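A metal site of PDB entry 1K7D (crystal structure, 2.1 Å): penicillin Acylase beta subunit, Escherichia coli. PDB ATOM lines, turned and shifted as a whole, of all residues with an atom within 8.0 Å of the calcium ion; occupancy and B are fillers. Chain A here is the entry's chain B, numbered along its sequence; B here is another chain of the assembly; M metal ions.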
ATOM      1  N   GLY A  72      18.171  -5.510 -21.862  1.00  0.00           N
ATOM      2  CA  GLY A  72      18.397  -5.719 -20.445  1.00  0.00           C
ATOM      3  C   GLY A  72      17.115  -5.207 -19.750  1.00  0.00           C
ATOM      4  O   GLY A  72      16.270  -4.545 -20.366  1.00  0.00           O
ATOM      5  N   ASP A  73      16.940  -5.528 -18.477  1.00  0.00           N
ATOM      6  CA  ASP A  73      15.777  -5.051 -17.774  1.00  0.00           C
ATOM      7  C   ASP A  73      16.099  -3.760 -17.078  1.00  0.00           C
ATOM      8  O   ASP A  73      16.621  -3.795 -15.984  1.00  0.00           O
ATOM      9  CB  ASP A  73      15.327  -6.058 -16.727  1.00  0.00           C
ATOM     10  CG  ASP A  73      14.090  -5.596 -15.967  1.00  0.00           C
ATOM     11  OD1 ASP A  73      13.600  -4.449 -16.171  1.00  0.00           O
ATOM     12  OD2 ASP A  73      13.545  -6.333 -15.165  1.00  0.00           O
ATOM     13  N   ASP A  74      15.748  -2.635 -17.707  1.00  0.00           N
ATOM     14  CA  ASP A  74      16.061  -1.315 -17.179  1.00  0.00           C
ATOM     15  C   ASP A  74      14.746  -0.557 -16.827  1.00  0.00           C
ATOM     16  O   ASP A  74      14.726   0.658 -16.694  1.00  0.00           O
ATOM     17  CB  ASP A  74      16.899  -0.542 -18.209  1.00  0.00           C
ATOM     18  CG  ASP A  74      16.185  -0.317 -19.523  1.00  0.00           C
ATOM     19  OD1 ASP A  74      15.076  -0.878 -19.717  1.00  0.00           O
ATOM     20  OD2 ASP A  74      16.615   0.450 -20.414  1.00  0.00           O
ATOM     21  N   VAL A  75      13.679  -1.290 -16.597  1.00  0.00           N
ATOM     22  CA  VAL A  75      12.376  -0.677 -16.367  1.00  0.00           C
ATOM     23  C   VAL A  75      11.550  -1.501 -15.325  1.00  0.00           C
ATOM     24  O   VAL A  75      11.333  -2.708 -15.475  1.00  0.00           O
ATOM     25  CB  VAL A  75      11.592  -0.592 -17.693  1.00  0.00           C
ATOM     26  CG1 VAL A  75      10.172  -0.173 -17.440  1.00  0.00           C
ATOM     27  CG2 VAL A  75      12.229   0.429 -18.697  1.00  0.00           C
ATOM     28  N   ASP A  76      11.105  -0.845 -14.259  1.00  0.00           N
ATOM     29  CA  ASP A  76      10.266  -1.500 -13.284  1.00  0.00           C
ATOM     30  C   ASP A  76       9.002  -0.702 -13.048  1.00  0.00           C
ATOM     31  O   ASP A  76       8.923   0.492 -13.372  1.00  0.00           O
ATOM     32  CB  ASP A  76      10.990  -1.642 -11.937  1.00  0.00           C
ATOM     33  CG  ASP A  76      12.195  -2.549 -11.986  1.00  0.00           C
ATOM     34  OD1 ASP A  76      12.306  -3.488 -12.847  1.00  0.00           O
ATOM     35  OD2 ASP A  76      13.123  -2.366 -11.138  1.00  0.00           O
ATOM     36  N   ILE A  77       8.030  -1.338 -12.421  1.00  0.00           N
ATOM     37  CA  ILE A  77       6.743  -0.738 -12.145  1.00  0.00           C
ATOM     38  C   ILE A  77       6.467  -0.685 -10.646  1.00  0.00           C
ATOM     39  O   ILE A  77       6.496  -1.725  -9.970  1.00  0.00           O
ATOM     40  CB  ILE A  77       5.629  -1.563 -12.836  1.00  0.00           C
ATOM     41  CG1 ILE A  77       5.657  -1.325 -14.340  1.00  0.00           C
ATOM     42  CG2 ILE A  77       4.256  -1.237 -12.229  1.00  0.00           C
ATOM     43  CD1 ILE A  77       4.604  -1.966 -15.035  1.00  0.00           C
ATOM     44  N   SER A 140       8.917   3.124 -14.127  1.00  0.00           N
ATOM     45  CA  SER A 140      10.217   3.649 -13.791  1.00  0.00           C
ATOM     46  C   SER A 140      11.291   3.162 -14.714  1.00  0.00           C
ATOM     47  O   SER A 140      11.520   1.945 -14.795  1.00  0.00           O
ATOM     48  CB  SER A 140      10.593   3.213 -12.375  1.00  0.00           C
ATOM     49  OG  SER A 140      11.561   4.108 -11.871  1.00  0.00           O
ATOM     50  N   PRO A 197      19.179  -0.309 -12.676  1.00  0.00           N
ATOM     51  CA  PRO A 197      18.883  -0.075 -11.258  1.00  0.00           C
ATOM     52  C   PRO A 197      19.705  -0.962 -10.346  1.00  0.00           C
ATOM     53  O   PRO A 197      19.992  -2.080 -10.673  1.00  0.00           O
ATOM     54  CB  PRO A 197      17.391  -0.422 -11.126  1.00  0.00           C
ATOM     55  CG  PRO A 197      17.192  -1.406 -12.205  1.00  0.00           C
ATOM     56  CD  PRO A 197      18.001  -0.854 -13.370  1.00  0.00           C
ATOM     57  N   ARG A 199      18.895  -2.582  -7.323  1.00  0.00           N
ATOM     58  CA  ARG A 199      17.637  -2.863  -6.593  1.00  0.00           C
ATOM     59  C   ARG A 199      17.853  -3.335  -5.169  1.00  0.00           C
ATOM     60  O   ARG A 199      18.952  -3.823  -4.842  1.00  0.00           O
ATOM     61  CB  ARG A 199      16.836  -3.938  -7.318  1.00  0.00           C
ATOM     62  CG  ARG A 199      16.516  -3.603  -8.777  1.00  0.00           C
ATOM     63  CD  ARG A 199      15.825  -4.751  -9.491  1.00  0.00           C
ATOM     64  NE  ARG A 199      15.260  -4.348 -10.786  1.00  0.00           N
ATOM     65  CZ  ARG A 199      15.866  -4.490 -11.951  1.00  0.00           C
ATOM     66  NH1 ARG A 199      17.104  -4.951 -12.028  1.00  0.00           N
ATOM     67  NH2 ARG A 199      15.236  -4.136 -13.050  1.00  0.00           N
ATOM     68  N   HIS A 203      14.262  -7.819  -4.487  1.00  0.00           N
ATOM     69  CA  HIS A 203      13.434  -7.241  -5.542  1.00  0.00           C
ATOM     70  C   HIS A 203      13.503  -8.145  -6.781  1.00  0.00           C
ATOM     71  O   HIS A 203      14.536  -8.247  -7.428  1.00  0.00           O
ATOM     72  CB  HIS A 203      13.934  -5.802  -5.820  1.00  0.00           C
ATOM     73  CG  HIS A 203      13.183  -5.037  -6.866  1.00  0.00           C
ATOM     74  ND1 HIS A 203      13.182  -3.664  -6.916  1.00  0.00           N
ATOM     75  CD2 HIS A 203      12.437  -5.440  -7.928  1.00  0.00           C
ATOM     76  CE1 HIS A 203      12.475  -3.252  -7.953  1.00  0.00           C
ATOM     77  NE2 HIS A 203      12.019  -4.322  -8.586  1.00  0.00           N
ATOM     78  N   ASP A 204      12.387  -8.817  -7.084  1.00  0.00           N
ATOM     79  CA  ASP A 204      12.219  -9.662  -8.277  1.00  0.00           C
ATOM     80  C   ASP A 204      11.829  -8.724  -9.410  1.00  0.00           C
ATOM     81  O   ASP A 204      10.738  -8.187  -9.414  1.00  0.00           O
ATOM     82  CB  ASP A 204      11.104 -10.680  -8.052  1.00  0.00           C
ATOM     83  CG  ASP A 204      10.998 -11.721  -9.166  1.00  0.00           C
ATOM     84  OD1 ASP A 204      11.411 -11.449 -10.319  1.00  0.00           O
ATOM     85  OD2 ASP A 204      10.524 -12.854  -8.984  1.00  0.00           O
ATOM     86  N   PRO A 205      12.705  -8.459 -10.359  1.00  0.00           N
ATOM     87  CA  PRO A 205      12.393  -7.415 -11.343  1.00  0.00           C
ATOM     88  C   PRO A 205      11.453  -7.817 -12.473  1.00  0.00           C
ATOM     89  O   PRO A 205      11.333  -7.089 -13.427  1.00  0.00           O
ATOM     90  CB  PRO A 205      13.775  -7.060 -11.892  1.00  0.00           C
ATOM     91  CG  PRO A 205      14.425  -8.380 -11.963  1.00  0.00           C
ATOM     92  CD  PRO A 205      14.051  -9.025 -10.587  1.00  0.00           C
ATOM     93  N   ARG A 206      10.865  -8.986 -12.368  1.00  0.00           N
ATOM     94  CA  ARG A 206       9.900  -9.465 -13.310  1.00  0.00           C
ATOM     95  C   ARG A 206       8.506  -9.068 -12.834  1.00  0.00           C
ATOM     96  O   ARG A 206       7.524  -9.247 -13.573  1.00  0.00           O
ATOM     97  CB  ARG A 206       9.967 -10.986 -13.384  1.00  0.00           C
ATOM     98  CG  ARG A 206      11.263 -11.605 -13.822  1.00  0.00           C
ATOM     99  CD  ARG A 206      11.282 -13.152 -13.677  1.00  0.00           C
ATOM    100  NE  ARG A 206      11.174 -13.590 -12.285  1.00  0.00           N
ATOM    101  CZ  ARG A 206      11.138 -14.847 -11.890  1.00  0.00           C
ATOM    102  NH1 ARG A 206      11.218 -15.849 -12.764  1.00  0.00           N
ATOM    103  NH2 ARG A 206      11.040 -15.125 -10.592  1.00  0.00           N
ATOM    104  N   LEU A 207       8.439  -8.511 -11.629  1.00  0.00           N
ATOM    105  CA  LEU A 207       7.160  -8.189 -11.005  1.00  0.00           C
ATOM    106  C   LEU A 207       7.126  -6.811 -10.394  1.00  0.00           C
ATOM    107  O   LEU A 207       8.143  -6.331  -9.934  1.00  0.00           O
ATOM    108  CB  LEU A 207       6.860  -9.229  -9.911  1.00  0.00           C
ATOM    109  CG  LEU A 207       6.956 -10.711 -10.307  1.00  0.00           C
ATOM    110  CD1 LEU A 207       6.791 -11.597  -9.094  1.00  0.00           C
ATOM    111  CD2 LEU A 207       5.900 -11.068 -11.264  1.00  0.00           C
ATOM    112  N   PRO A 208       5.962  -6.160 -10.336  1.00  0.00           N
ATOM    113  CA  PRO A 208       5.869  -4.825  -9.724  1.00  0.00           C
ATOM    114  C   PRO A 208       6.266  -4.831  -8.271  1.00  0.00           C
ATOM    115  O   PRO A 208       6.260  -5.899  -7.688  1.00  0.00           O
ATOM    116  CB  PRO A 208       4.397  -4.486  -9.828  1.00  0.00           C
ATOM    117  CG  PRO A 208       3.886  -5.391 -10.870  1.00  0.00           C
ATOM    118  CD  PRO A 208       4.655  -6.632 -10.801  1.00  0.00           C
ATOM    119  N   TRP A 217      14.521   1.844  -5.688  1.00  0.00           N
ATOM    120  CA  TRP A 217      15.893   1.624  -6.116  1.00  0.00           C
ATOM    121  C   TRP A 217      16.883   2.385  -5.201  1.00  0.00           C
ATOM    122  O   TRP A 217      16.576   3.467  -4.718  1.00  0.00           O
ATOM    123  CB  TRP A 217      16.030   2.163  -7.533  1.00  0.00           C
ATOM    124  CG  TRP A 217      15.261   1.401  -8.614  1.00  0.00           C
ATOM    125  CD1 TRP A 217      14.669   0.158  -8.519  1.00  0.00           C
ATOM    126  CD2 TRP A 217      15.049   1.838  -9.957  1.00  0.00           C
ATOM    127  NE1 TRP A 217      14.115  -0.183  -9.726  1.00  0.00           N
ATOM    128  CE2 TRP A 217      14.352   0.821 -10.630  1.00  0.00           C
ATOM    129  CE3 TRP A 217      15.414   2.989 -10.670  1.00  0.00           C
ATOM    130  CZ2 TRP A 217      13.967   0.941 -11.981  1.00  0.00           C
ATOM    131  CZ3 TRP A 217      15.037   3.111 -12.014  1.00  0.00           C
ATOM    132  CH2 TRP A 217      14.298   2.072 -12.649  1.00  0.00           C
ATOM    133  N   ALA A 250      17.791 -10.933 -18.622  1.00  0.00           N
ATOM    134  CA  ALA A 250      17.081 -10.268 -19.695  1.00  0.00           C
ATOM    135  C   ALA A 250      15.919  -9.374 -19.272  1.00  0.00           C
ATOM    136  O   ALA A 250      15.435  -9.433 -18.129  1.00  0.00           O
ATOM    137  CB  ALA A 250      16.477 -11.326 -20.609  1.00  0.00           C
ATOM    138  N   SER A 251      15.458  -8.580 -20.229  1.00  0.00           N
ATOM    139  CA  SER A 251      14.203  -7.826 -20.087  1.00  0.00           C
ATOM    140  C   SER A 251      13.143  -8.653 -19.345  1.00  0.00           C
ATOM    141  O   SER A 251      13.086  -9.884 -19.477  1.00  0.00           O
ATOM    142  CB  SER A 251      13.680  -7.562 -21.479  1.00  0.00           C
ATOM    143  OG  SER A 251      12.382  -7.012 -21.475  1.00  0.00           O
ATOM    144  N   ASP A 252      12.228  -7.985 -18.634  1.00  0.00           N
ATOM    145  CA  ASP A 252      11.185  -8.738 -17.913  1.00  0.00           C
ATOM    146  C   ASP A 252      10.007  -9.138 -18.809  1.00  0.00           C
ATOM    147  O   ASP A 252       9.073  -9.809 -18.328  1.00  0.00           O
ATOM    148  CB  ASP A 252      10.690  -7.990 -16.683  1.00  0.00           C
ATOM    149  CG  ASP A 252      10.013  -6.631 -17.042  1.00  0.00           C
ATOM    150  OD1 ASP A 252       9.193  -6.611 -17.969  1.00  0.00           O
ATOM    151  OD2 ASP A 252      10.302  -5.566 -16.460  1.00  0.00           O
ATOM    152  N   LEU A 253      10.029  -8.751 -20.089  1.00  0.00           N
ATOM    153  CA  LEU A 253       8.951  -9.107 -21.036  1.00  0.00           C
ATOM    154  C   LEU A 253       8.630 -10.592 -21.097  1.00  0.00           C
ATOM    155  O   LEU A 253       9.492 -11.374 -21.472  1.00  0.00           O
ATOM    156  CB  LEU A 253       9.318  -8.730 -22.485  1.00  0.00           C
ATOM    157  CG  LEU A 253       9.318  -7.241 -22.749  1.00  0.00           C
ATOM    158  CD1 LEU A 253       9.782  -6.994 -24.128  1.00  0.00           C
ATOM    159  CD2 LEU A 253       7.943  -6.645 -22.556  1.00  0.00           C
ATOM    160  N   SER B 150      10.649  -1.059 -22.267  1.00  0.00           N
ATOM    161  CA  SER B 150       9.886  -2.289 -22.270  1.00  0.00           C
ATOM    162  C   SER B 150       9.670  -2.924 -20.942  1.00  0.00           C
ATOM    163  O   SER B 150      10.644  -3.267 -20.297  1.00  0.00           O
ATOM    164  CB  SER B 150      10.642  -3.335 -23.087  1.00  0.00           C
ATOM    165  OG  SER B 150      10.696  -2.946 -24.436  1.00  0.00           O
ATOM    166  N   THR B 151       8.423  -3.123 -20.569  1.00  0.00           N
ATOM    167  CA  THR B 151       8.106  -3.906 -19.386  1.00  0.00           C
ATOM    168  C   THR B 151       6.773  -4.615 -19.550  1.00  0.00           C
ATOM    169  O   THR B 151       5.913  -4.144 -20.263  1.00  0.00           O
ATOM    170  CB  THR B 151       8.058  -3.060 -18.143  1.00  0.00           C
ATOM    171  OG1 THR B 151       7.971  -3.926 -17.009  1.00  0.00           O
ATOM    172  CG2 THR B 151       6.742  -2.258 -18.080  1.00  0.00           C
ATOM    173  N   SER B 152       6.601  -5.773 -18.907  1.00  0.00           N
ATOM    174  CA  SER B 152       5.279  -6.465 -18.854  1.00  0.00           C
ATOM    175  C   SER B 152       5.013  -6.940 -17.439  1.00  0.00           C
ATOM    176  O   SER B 152       4.328  -7.944 -17.240  1.00  0.00           O
ATOM    177  CB  SER B 152       5.185  -7.650 -19.809  1.00  0.00           C
ATOM    178  OG  SER B 152       6.093  -8.704 -19.509  1.00  0.00           O
ATOM    179  N   GLU B 153       5.506  -6.189 -16.467  1.00  0.00           N
ATOM    180  CA  GLU B 153       5.438  -6.635 -15.074  1.00  0.00           C
ATOM    181  C   GLU B 153       4.019  -6.853 -14.574  1.00  0.00           C
ATOM    182  O   GLU B 153       3.799  -7.797 -13.844  1.00  0.00           O
ATOM    183  CB  GLU B 153       6.171  -5.677 -14.134  1.00  0.00           C
ATOM    184  CG  GLU B 153       7.654  -5.611 -14.333  1.00  0.00           C
ATOM    185  CD  GLU B 153       8.368  -4.730 -13.307  1.00  0.00           C
ATOM    186  OE1 GLU B 153       7.683  -4.179 -12.405  1.00  0.00           O
ATOM    187  OE2 GLU B 153       9.581  -4.553 -13.448  1.00  0.00           O
ATOM    188  N   ASN B 156       3.018 -10.049 -16.049  1.00  0.00           N
ATOM    189  CA  ASN B 156       3.761 -11.120 -15.442  1.00  0.00           C
ATOM    190  C   ASN B 156       3.149 -11.529 -14.102  1.00  0.00           C
ATOM    191  O   ASN B 156       3.079 -12.730 -13.788  1.00  0.00           O
ATOM    192  CB  ASN B 156       5.210 -10.723 -15.237  1.00  0.00           C
ATOM    193  CG  ASN B 156       5.951 -10.414 -16.551  1.00  0.00           C
ATOM    194  OD1 ASN B 156       5.470 -10.684 -17.657  1.00  0.00           O
ATOM    195  ND2 ASN B 156       7.163  -9.838 -16.419  1.00  0.00           N
HETATM  196 CA    CA M   1      11.519  -4.954 -14.501  1.00  0.00          CA
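The calcium ion is bound by OE2 of Glu 153 of chain B (2.2 Å), OD1 of Asp 76 (2.3 Å), OD2 of Asp 252 (2.4 Å), O of Pro 205 (2.4 Å), O of Val 75 (2.5 Å), OD2 of Asp 73 (2.5 Å) and OD1 of Asp 73 (2.7 Å). The calcium ion has seven donor atoms within binding distance.
Within 4 Å of the calcium ion: Asp 73, Val 75, Asp 76, Pro 205, Asp 252 and Glu 153 of chain B.
N of Glu 153 of chain B lies close to OG1 of Thr 151 of chain B (3.4 Å). N of Ile 77 sits at hydrogen-bond distance from OE1 of Glu 153 of chain B, at 2.9 Å. The side-chain carboxylate of Asp 76 lies within salt-bridge range of the guanidinium group of Arg 199, 2.9 Å away. NE2 of His 203 sits close to OD2 of Asp 76 (3.4 Å). The backbone NH (N) of Ser 140 lies within hydrogen-bond range of the backbone carbonyl oxygen (O) of Asp 76 (2.7 Å). OD1 of Asp 252 sits at hydrogen-bond distance from OG1 of Thr 151 of chain B (3.1 Å). OD1 of Asp 252 is in hydrogen-bond range of N of Ser 152 of chain B, 2.9 Å away. The backbone carbonyl oxygen of Asp 252 is in hydrogen-bond range of the side-chain amide nitrogen of Asn 156 of chain B (2.7 Å).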
